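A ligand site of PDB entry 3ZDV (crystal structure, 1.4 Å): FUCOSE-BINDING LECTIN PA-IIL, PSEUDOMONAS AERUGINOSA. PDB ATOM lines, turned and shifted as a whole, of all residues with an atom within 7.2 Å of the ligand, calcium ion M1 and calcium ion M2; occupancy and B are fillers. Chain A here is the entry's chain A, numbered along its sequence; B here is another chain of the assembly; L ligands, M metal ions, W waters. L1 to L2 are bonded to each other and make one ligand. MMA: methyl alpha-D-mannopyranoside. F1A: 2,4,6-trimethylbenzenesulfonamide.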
ATOM      1  N   ALA A  21     -21.181 -20.034  11.260  1.00  0.00           N
ATOM      2  CA  ALA A  21     -20.912 -20.377  12.660  1.00  0.00           C
ATOM      3  C   ALA A  21     -19.792 -21.398  12.827  1.00  0.00           C
ATOM      4  O   ALA A  21     -19.695 -22.337  12.045  1.00  0.00           O
ATOM      5  CB  ALA A  21     -22.181 -20.853  13.348  1.00  0.00           C
ATOM      6  N   ASN A  22     -18.949 -21.170  13.860  1.00  0.00           N
ATOM      7  CA  ASN A  22     -17.859 -22.057  14.193  1.00  0.00           C
ATOM      8  C   ASN A  22     -17.657 -22.068  15.699  1.00  0.00           C
ATOM      9  O   ASN A  22     -16.687 -21.507  16.223  1.00  0.00           O
ATOM     10  CB  ASN A  22     -16.554 -21.624  13.530  1.00  0.00           C
ATOM     11  CG  ASN A  22     -16.559 -21.790  12.046  1.00  0.00           C
ATOM     12  OD1 ASN A  22     -16.374 -22.883  11.522  1.00  0.00           O
ATOM     13  ND2 ASN A  22     -16.797 -20.671  11.336  1.00  0.00           N
ATOM     14  N   SER A  23     -18.595 -22.674  16.407  1.00  0.00           N
ATOM     15  CA  SER A  23     -18.615 -22.610  17.852  1.00  0.00           C
ATOM     16  C   SER A  23     -19.531 -23.663  18.435  1.00  0.00           C
ATOM     17  O   SER A  23     -20.544 -24.017  17.833  1.00  0.00           O
ATOM     18  CB  SER A  23     -19.117 -21.232  18.305  1.00  0.00           C
ATOM     19  OG  SER A  23     -19.208 -21.178  19.732  1.00  0.00           O
ATOM     20  N   SER A  24     -19.229 -24.111  19.646  1.00  0.00           N
ATOM     21  CA  SER A  24     -20.173 -24.940  20.391  1.00  0.00           C
ATOM     22  C   SER A  24     -21.425 -24.210  20.821  1.00  0.00           C
ATOM     23  O   SER A  24     -22.470 -24.844  21.077  1.00  0.00           O
ATOM     24  CB  SER A  24     -19.470 -25.523  21.624  1.00  0.00           C
ATOM     25  OG  SER A  24     -18.422 -26.395  21.277  1.00  0.00           O
ATOM     26  N   GLY A  25     -21.326 -22.894  20.939  1.00  0.00           N
ATOM     27  CA  GLY A  25     -22.472 -22.110  21.313  1.00  0.00           C
ATOM     28  C   GLY A  25     -23.338 -21.610  20.157  1.00  0.00           C
ATOM     29  O   GLY A  25     -22.838 -21.376  19.071  1.00  0.00           O
ATOM     30  N   THR A  26     -24.654 -21.518  20.359  1.00  0.00           N
ATOM     31  CA  THR A  26     -25.574 -21.006  19.376  1.00  0.00           C
ATOM     32  C   THR A  26     -25.315 -19.523  19.210  1.00  0.00           C
ATOM     33  O   THR A  26     -25.280 -18.764  20.164  1.00  0.00           O
ATOM     34  CB  THR A  26     -27.039 -21.266  19.795  1.00  0.00           C
ATOM     35  OG1 THR A  26     -27.240 -22.668  19.857  1.00  0.00           O
ATOM     36  CG2 THR A  26     -27.977 -20.633  18.845  1.00  0.00           C
ATOM     37  N   GLN A  27     -25.094 -19.142  17.966  1.00  0.00           N
ATOM     38  CA  GLN A  27     -24.801 -17.726  17.655  1.00  0.00           C
ATOM     39  C   GLN A  27     -26.072 -17.012  17.309  1.00  0.00           C
ATOM     40  O   GLN A  27     -26.880 -17.578  16.555  1.00  0.00           O
ATOM     41  CB  GLN A  27     -23.883 -17.676  16.464  1.00  0.00           C
ATOM     42  CG  GLN A  27     -22.603 -18.460  16.665  1.00  0.00           C
ATOM     43  CD  GLN A  27     -21.723 -17.889  17.754  1.00  0.00           C
ATOM     44  OE1 GLN A  27     -21.377 -16.729  17.742  1.00  0.00           O
ATOM     45  NE2 GLN A  27     -21.326 -18.744  18.690  1.00  0.00           N
ATOM     46  N   SER A  45     -23.113 -24.329  14.631  1.00  0.00           N
ATOM     47  CA  SER A  45     -22.288 -25.205  13.824  1.00  0.00           C
ATOM     48  C   SER A  45     -20.833 -25.084  14.259  1.00  0.00           C
ATOM     49  O   SER A  45     -20.423 -23.998  14.698  1.00  0.00           O
ATOM     50  CB  SER A  45     -22.335 -24.786  12.356  1.00  0.00           C
ATOM     51  OG  SER A  45     -21.509 -25.586  11.528  1.00  0.00           O
ATOM     52  N   THR A  46     -20.074 -26.170  14.154  1.00  0.00           N
ATOM     53  CA  THR A  46     -18.617 -26.108  14.267  1.00  0.00           C
ATOM     54  C   THR A  46     -17.948 -26.410  12.941  1.00  0.00           C
ATOM     55  O   THR A  46     -16.747 -26.661  12.898  1.00  0.00           O
ATOM     56  CB  THR A  46     -18.076 -27.062  15.332  1.00  0.00           C
ATOM     57  OG1 THR A  46     -18.592 -28.370  15.132  1.00  0.00           O
ATOM     58  CG2 THR A  46     -18.413 -26.521  16.728  1.00  0.00           C
ATOM     59  N   VAL A  70     -24.182 -14.728  22.307  1.00  0.00           N
ATOM     60  CA  VAL A  70     -24.326 -16.170  22.573  1.00  0.00           C
ATOM     61  C   VAL A  70     -24.953 -16.293  23.943  1.00  0.00           C
ATOM     62  O   VAL A  70     -24.411 -15.772  24.933  1.00  0.00           O
ATOM     63  CB  VAL A  70     -22.972 -16.877  22.559  1.00  0.00           C
ATOM     64  CG1 VAL A  70     -23.162 -18.338  22.918  1.00  0.00           C
ATOM     65  CG2 VAL A  70     -22.333 -16.709  21.211  1.00  0.00           C
ATOM     66  N   ASN A  71     -26.117 -16.923  23.992  1.00  0.00           N
ATOM     67  CA  ASN A  71     -26.933 -16.985  25.216  1.00  0.00           C
ATOM     68  C   ASN A  71     -27.046 -15.644  25.905  1.00  0.00           C
ATOM     69  O   ASN A  71     -26.963 -15.553  27.137  1.00  0.00           O
ATOM     70  CB  ASN A  71     -26.375 -18.065  26.153  1.00  0.00           C
ATOM     71  CG  ASN A  71     -26.350 -19.444  25.486  1.00  0.00           C
ATOM     72  OD1 ASN A  71     -25.522 -20.280  25.821  1.00  0.00           O
ATOM     73  ND2 ASN A  71     -27.229 -19.683  24.512  1.00  0.00           N
ATOM     74  N   SER A  95     -15.992 -12.715  15.472  1.00  0.00           N
ATOM     75  CA  SER A  95     -16.491 -12.559  16.828  1.00  0.00           C
ATOM     76  C   SER A  95     -15.988 -13.719  17.690  1.00  0.00           C
ATOM     77  O   SER A  95     -15.755 -14.825  17.196  1.00  0.00           O
ATOM     78  CB  SER A  95     -18.004 -12.515  16.856  1.00  0.00           C
ATOM     79  OG  SER A  95     -18.584 -13.713  16.431  1.00  0.00           O
ATOM     80  N   GLU A  96     -15.782 -13.410  18.969  1.00  0.00           N
ATOM     81  CA  GLU A  96     -15.259 -14.362  19.927  1.00  0.00           C
ATOM     82  C   GLU A  96     -16.182 -14.468  21.129  1.00  0.00           C
ATOM     83  O   GLU A  96     -16.501 -13.462  21.769  1.00  0.00           O
ATOM     84  CB  GLU A  96     -13.853 -13.908  20.417  1.00  0.00           C
ATOM     85  CG  GLU A  96     -13.229 -14.858  21.425  1.00  0.00           C
ATOM     86  CD  GLU A  96     -13.160 -16.279  20.955  1.00  0.00           C
ATOM     87  OE1 GLU A  96     -12.682 -16.554  19.823  1.00  0.00           O
ATOM     88  OE2 GLU A  96     -13.628 -17.186  21.697  1.00  0.00           O
ATOM     89  N   ASP A  97     -16.608 -15.702  21.400  1.00  0.00           N
ATOM     90  CA  ASP A  97     -17.544 -15.977  22.490  1.00  0.00           C
ATOM     91  C   ASP A  97     -16.912 -16.687  23.696  1.00  0.00           C
ATOM     92  O   ASP A  97     -17.628 -16.997  24.647  1.00  0.00           O
ATOM     93  CB  ASP A  97     -18.737 -16.784  21.965  1.00  0.00           C
ATOM     94  CG  ASP A  97     -18.372 -18.140  21.470  1.00  0.00           C
ATOM     95  OD1 ASP A  97     -17.318 -18.682  21.895  1.00  0.00           O
ATOM     96  OD2 ASP A  97     -19.183 -18.749  20.723  1.00  0.00           O
ATOM     97  N   GLY A  98     -15.627 -16.942  23.660  1.00  0.00           N
ATOM     98  CA  GLY A  98     -14.927 -17.763  24.637  1.00  0.00           C
ATOM     99  C   GLY A  98     -13.531 -17.260  24.905  1.00  0.00           C
ATOM    100  O   GLY A  98     -13.278 -16.066  24.987  1.00  0.00           O
ATOM    101  N   THR A  99     -12.604 -18.212  25.029  1.00  0.00           N
ATOM    102  CA  THR A  99     -11.254 -17.917  25.478  1.00  0.00           C
ATOM    103  C   THR A  99     -10.160 -18.216  24.473  1.00  0.00           C
ATOM    104  O   THR A  99      -9.011 -17.835  24.672  1.00  0.00           O
ATOM    105  CB  THR A  99     -10.908 -18.665  26.786  1.00  0.00           C
ATOM    106  OG1 THR A  99     -10.970 -20.065  26.518  1.00  0.00           O
ATOM    107  CG2 THR A  99     -11.866 -18.300  27.865  1.00  0.00           C
ATOM    108  N   ASP A 100     -10.477 -18.901  23.367  1.00  0.00           N
ATOM    109  CA  ASP A 100      -9.431 -19.365  22.450  1.00  0.00           C
ATOM    110  C   ASP A 100      -8.978 -18.323  21.446  1.00  0.00           C
ATOM    111  O   ASP A 100      -7.979 -18.520  20.757  1.00  0.00           O
ATOM    112  CB  ASP A 100      -9.811 -20.672  21.799  1.00  0.00           C
ATOM    113  CG  ASP A 100     -10.946 -20.534  20.804  1.00  0.00           C
ATOM    114  OD1 ASP A 100     -11.634 -19.481  20.767  1.00  0.00           O
ATOM    115  OD2 ASP A 100     -11.184 -21.552  20.046  1.00  0.00           O
ATOM    116  N   ASN A 101      -9.712 -17.227  21.342  1.00  0.00           N
ATOM    117  CA  ASN A 101      -9.383 -16.117  20.426  1.00  0.00           C
ATOM    118  C   ASN A 101      -9.205 -16.536  18.979  1.00  0.00           C
ATOM    119  O   ASN A 101      -8.340 -15.998  18.278  1.00  0.00           O
ATOM    120  CB  ASN A 101      -8.185 -15.316  20.956  1.00  0.00           C
ATOM    121  CG  ASN A 101      -8.494 -14.661  22.243  1.00  0.00           C
ATOM    122  OD1 ASN A 101      -9.680 -14.399  22.591  1.00  0.00           O
ATOM    123  ND2 ASN A 101      -7.462 -14.468  23.036  1.00  0.00           N
ATOM    124  N   ASP A 102     -10.008 -17.466  18.501  1.00  0.00           N
ATOM    125  CA  ASP A 102     -10.056 -17.756  17.075  1.00  0.00           C
ATOM    126  C   ASP A 102     -10.892 -16.728  16.287  1.00  0.00           C
ATOM    127  O   ASP A 102     -10.715 -16.602  15.076  1.00  0.00           O
ATOM    128  CB  ASP A 102     -10.432 -19.219  16.727  1.00  0.00           C
ATOM    129  CG  ASP A 102     -11.817 -19.692  17.186  1.00  0.00           C
ATOM    130  OD1 ASP A 102     -12.581 -18.892  17.792  1.00  0.00           O
ATOM    131  OD2 ASP A 102     -12.122 -20.863  16.874  1.00  0.00           O
ATOM    132  N   TYR A 103     -11.801 -16.017  16.982  1.00  0.00           N
ATOM    133  CA  TYR A 103     -12.612 -14.959  16.349  1.00  0.00           C
ATOM    134  C   TYR A 103     -13.446 -15.407  15.179  1.00  0.00           C
ATOM    135  O   TYR A 103     -13.816 -14.593  14.348  1.00  0.00           O
ATOM    136  CB  TYR A 103     -11.743 -13.707  16.075  1.00  0.00           C
ATOM    137  CG  TYR A 103     -11.573 -12.908  17.345  1.00  0.00           C
ATOM    138  CD1 TYR A 103     -10.586 -13.184  18.231  1.00  0.00           C
ATOM    139  CD2 TYR A 103     -12.496 -11.887  17.675  1.00  0.00           C
ATOM    140  CE1 TYR A 103     -10.489 -12.507  19.446  1.00  0.00           C
ATOM    141  CE2 TYR A 103     -12.404 -11.158  18.864  1.00  0.00           C
ATOM    142  CZ  TYR A 103     -11.395 -11.534  19.758  1.00  0.00           C
ATOM    143  OH  TYR A 103     -11.309 -10.892  20.996  1.00  0.00           O
ATOM    144  N   ASN A 104     -13.790 -16.683  15.125  1.00  0.00           N
ATOM    145  CA  ASN A 104     -14.567 -17.245  14.022  1.00  0.00           C
ATOM    146  C   ASN A 104     -15.941 -17.745  14.475  1.00  0.00           C
ATOM    147  O   ASN A 104     -16.626 -18.420  13.748  1.00  0.00           O
ATOM    148  CB  ASN A 104     -13.816 -18.365  13.325  1.00  0.00           C
ATOM    149  CG  ASN A 104     -13.724 -19.623  14.193  1.00  0.00           C
ATOM    150  OD1 ASN A 104     -14.256 -19.643  15.286  1.00  0.00           O
ATOM    151  ND2 ASN A 104     -13.115 -20.692  13.655  1.00  0.00           N
ATOM    152  N   ASP A 105     -16.308 -17.424  15.715  1.00  0.00           N
ATOM    153  CA  ASP A 105     -17.425 -18.122  16.326  1.00  0.00           C
ATOM    154  C   ASP A 105     -18.722 -17.803  15.602  1.00  0.00           C
ATOM    155  O   ASP A 105     -19.508 -18.713  15.329  1.00  0.00           O
ATOM    156  CB  ASP A 105     -17.466 -17.785  17.818  1.00  0.00           C
ATOM    157  CG  ASP A 105     -16.205 -18.274  18.540  1.00  0.00           C
ATOM    158  OD1 ASP A 105     -15.656 -19.340  18.188  1.00  0.00           O
ATOM    159  OD2 ASP A 105     -15.757 -17.565  19.459  1.00  0.00           O
ATOM    160  N   ALA A 106     -18.896 -16.539  15.270  1.00  0.00           N
ATOM    161  CA  ALA A 106     -19.783 -16.124  14.142  1.00  0.00           C
ATOM    162  C   ALA A 106     -18.892 -15.266  13.248  1.00  0.00           C
ATOM    163  O   ALA A 106     -18.161 -14.376  13.732  1.00  0.00           O
ATOM    164  CB  ALA A 106     -20.994 -15.362  14.553  1.00  0.00           C
ATOM    165  N   PRO B 113      -9.405 -19.809  10.280  1.00  0.00           N
ATOM    166  CA  PRO B 113      -9.653 -21.229  10.580  1.00  0.00           C
ATOM    167  C   PRO B 113     -11.128 -21.451  10.892  1.00  0.00           C
ATOM    168  O   PRO B 113     -11.896 -20.514  11.085  1.00  0.00           O
ATOM    169  CB  PRO B 113      -8.840 -21.459  11.865  1.00  0.00           C
ATOM    170  CG  PRO B 113      -8.977 -20.151  12.556  1.00  0.00           C
ATOM    171  CD  PRO B 113      -8.889 -19.101  11.475  1.00  0.00           C
ATOM    172  N   LEU B 114     -11.517 -22.711  10.880  1.00  0.00           N
ATOM    173  CA  LEU B 114     -12.877 -23.151  11.192  1.00  0.00           C
ATOM    174  C   LEU B 114     -12.902 -23.810  12.576  1.00  0.00           C
ATOM    175  O   LEU B 114     -11.851 -23.993  13.186  1.00  0.00           O
ATOM    176  CB  LEU B 114     -13.377 -24.160  10.118  1.00  0.00           C
ATOM    177  CG  LEU B 114     -13.313 -23.630   8.691  1.00  0.00           C
ATOM    178  CD1 LEU B 114     -14.013 -24.644   7.784  1.00  0.00           C
ATOM    179  CD2 LEU B 114     -13.961 -22.247   8.513  1.00  0.00           C
ATOM    180  N   GLY B 115     -14.096 -24.137  13.041  1.00  0.00           N
ATOM    181  CA  GLY B 115     -14.318 -24.903  14.253  1.00  0.00           C
ATOM    182  C   GLY B 115     -14.473 -24.084  15.494  1.00  0.00           C
ATOM    183  O   GLY B 115     -14.062 -22.900  15.576  1.00  0.00           O
ATOM    184  OXT GLY B 115     -14.995 -24.659  16.494  1.00  0.00           O
HETATM  185  C1  MMA L   1     -15.489 -24.242  20.559  1.00  0.00           C
HETATM  186  C2  MMA L   1     -14.630 -23.394  19.666  1.00  0.00           C
HETATM  187  C3  MMA L   1     -14.281 -22.067  20.316  1.00  0.00           C
HETATM  188  C4  MMA L   1     -15.509 -21.386  20.827  1.00  0.00           C
HETATM  189  C5  MMA L   1     -16.205 -22.338  21.825  1.00  0.00           C
HETATM  190  C6  MMA L   1     -17.469 -21.779  22.446  1.00  0.00           C
HETATM  191  C7  MMA L   1     -15.259 -25.603  22.509  1.00  0.00           C
HETATM  192  O1  MMA L   1     -14.626 -24.682  21.590  1.00  0.00           O
HETATM  193  O2  MMA L   1     -15.356 -23.103  18.458  1.00  0.00           O
HETATM  194  O3  MMA L   1     -13.596 -21.244  19.359  1.00  0.00           O
HETATM  195  O4  MMA L   1     -15.183 -20.117  21.395  1.00  0.00           O
HETATM  196  O5  MMA L   1     -16.592 -23.506  21.072  1.00  0.00           O
HETATM  197  N   F1A L   2     -17.164 -20.904  23.568  1.00  0.00           N
HETATM  198  S   F1A L   2     -17.431 -21.486  25.072  1.00  0.00           S
HETATM  199  O1  F1A L   2     -17.304 -20.376  25.986  1.00  0.00           O
HETATM  200  O2  F1A L   2     -16.548 -22.601  25.211  1.00  0.00           O
HETATM  201  C1  F1A L   2     -19.030 -22.033  25.071  1.00  0.00           C
HETATM  202  C2  F1A L   2     -19.419 -23.461  25.099  1.00  0.00           C
HETATM  203  C3  F1A L   2     -20.751 -23.814  24.999  1.00  0.00           C
HETATM  204  C4  F1A L   2     -21.748 -22.879  24.921  1.00  0.00           C
HETATM  205  C5  F1A L   2     -21.478 -21.524  24.867  1.00  0.00           C
HETATM  206  C6  F1A L   2     -20.148 -21.092  24.953  1.00  0.00           C
HETATM  207  C7  F1A L   2     -18.430 -24.586  25.199  1.00  0.00           C
HETATM  208  C9  F1A L   2     -19.862 -19.619  24.878  1.00  0.00           C
HETATM  209  C8  F1A L   2     -23.179 -23.335  24.866  1.00  0.00           C
HETATM  210 CA    CA M   1     -13.678 -18.793  19.864  1.00  0.00          CA
HETATM  211 CA    CA M   2     -14.550 -21.095  17.086  1.00  0.00          CA
HETATM  212  O   HOH W   1     -15.435 -20.470  28.066  1.00  0.00           O
HETATM  213  O   HOH W   2     -13.193 -20.606  23.534  1.00  0.00           O
HETATM  214  O   HOH W   3     -17.566 -17.573  27.449  1.00  0.00           O
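N of Asn 22 lies close to O of Ser 45, 3.3 Å away.
The side-chain carboxylate of Asp 105 sits close to the backbone NH of Asp 97.
The side-chain hydroxyl (OG) of Ser 23 lies close to the side-chain amide nitrogen (NE2) of Gln 27 (3.4 Å).
The side-chain carboxylate (OE1) of Glu 96 sits close to the backbone NH (N) of Tyr 103 (3.0 Å).
O of Gly 25 is in hydrogen-bond range of NE2 of Gln 27 (3.1 Å).
The backbone NH of Gly 98 sits close to the side-chain carboxylate of Glu 96 (2.8 Å).
The backbone NH (N) of Asn 101 lies close to the side-chain carboxylate (OE1) of Glu 96.
The backbone carbonyl oxygen (O) of Pro 113 of chain B lies within hydrogen-bond range of the side-chain amide nitrogen (ND2) of Asn 104, at 2.9 Å.
Calcium ion M2 is bound by OD1 of Asn 104 (2.3 Å), O of Asn 22 (2.3 Å), OD1 of Asp 105 (2.3 Å), O of Gly 115 of chain B (2.4 Å), OD2 of Asp 102 (2.4 Å), O3 of MMA L1 (2.5 Å) and O2 of MMA L1 (2.6 Å).
Slightly farther from calcium ion M2 lies OD1 of Asp 102 (3.0 Å).
Water W3 bridges O of Asp 97 (2.9 Å) and O1 of F1A L2 (3.2 Å).
Five residues have an atom within 4 Å of calcium ion M2: Asn 22, Asp 102, Asn 104, Asp 105 and Gly 115 of chain B.
The nearest printed residue that does not touch calcium ion M2 is Ser 23 (4.4 Å).
Within 4 Å of calcium ion M1: Glu 96, Asp 100, Asp 102 and Asp 105.
OG of Ser 23 touches C6 of MMA L1 (3.3 Å).
CA of Gly 25 touches C5 of F1A L2, at 3.7 Å.
Asn 71 touches the ligand.
CA of Gly 98 touches O1 of F1A L2, at 3.8 Å.
Of the 26 residues printed, 12 come within 4 Å of the ligand.
Along chain A the residues within 4 Å of the ligand span positions 22 to 105.
The nearest printed residue that does not touch the ligand is Val 70 (4.05 Å).
The side-chain carboxylate of Asp 97 sits at hydrogen-bond distance from a nitrogen (N) of F1A L2, 2.8 Å away.
The side-chain hydroxyl of Ser 24 sits at hydrogen-bond distance from an oxygen (O5) of MMA L1 (3.4 Å).
N of Ser 24 sits at hydrogen-bond distance from O5 of MMA L1, 3.1 Å away.
Calcium ion M1 is bound by OD1 of Asp 100, at 2.3 Å.
OD1 of Asp 102 is bound to calcium ion M1 (2.3 Å).
Calcium ion M1 is bound by OE2 of Glu 96, at 2.4 Å.
OD2 of Asp 105 is bound to calcium ion M1, 2.4 Å away.
OE1 of Glu 96 is bound to calcium ion M1 (2.5 Å).
O3 of MMA L1 is bound to calcium ion M1 (2.5 Å).
O4 of MMA L1 is bound to calcium ion M1 (2.5 Å).
OD1 of Asp 105 is bound to calcium ion M1, 2.6 Å away.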
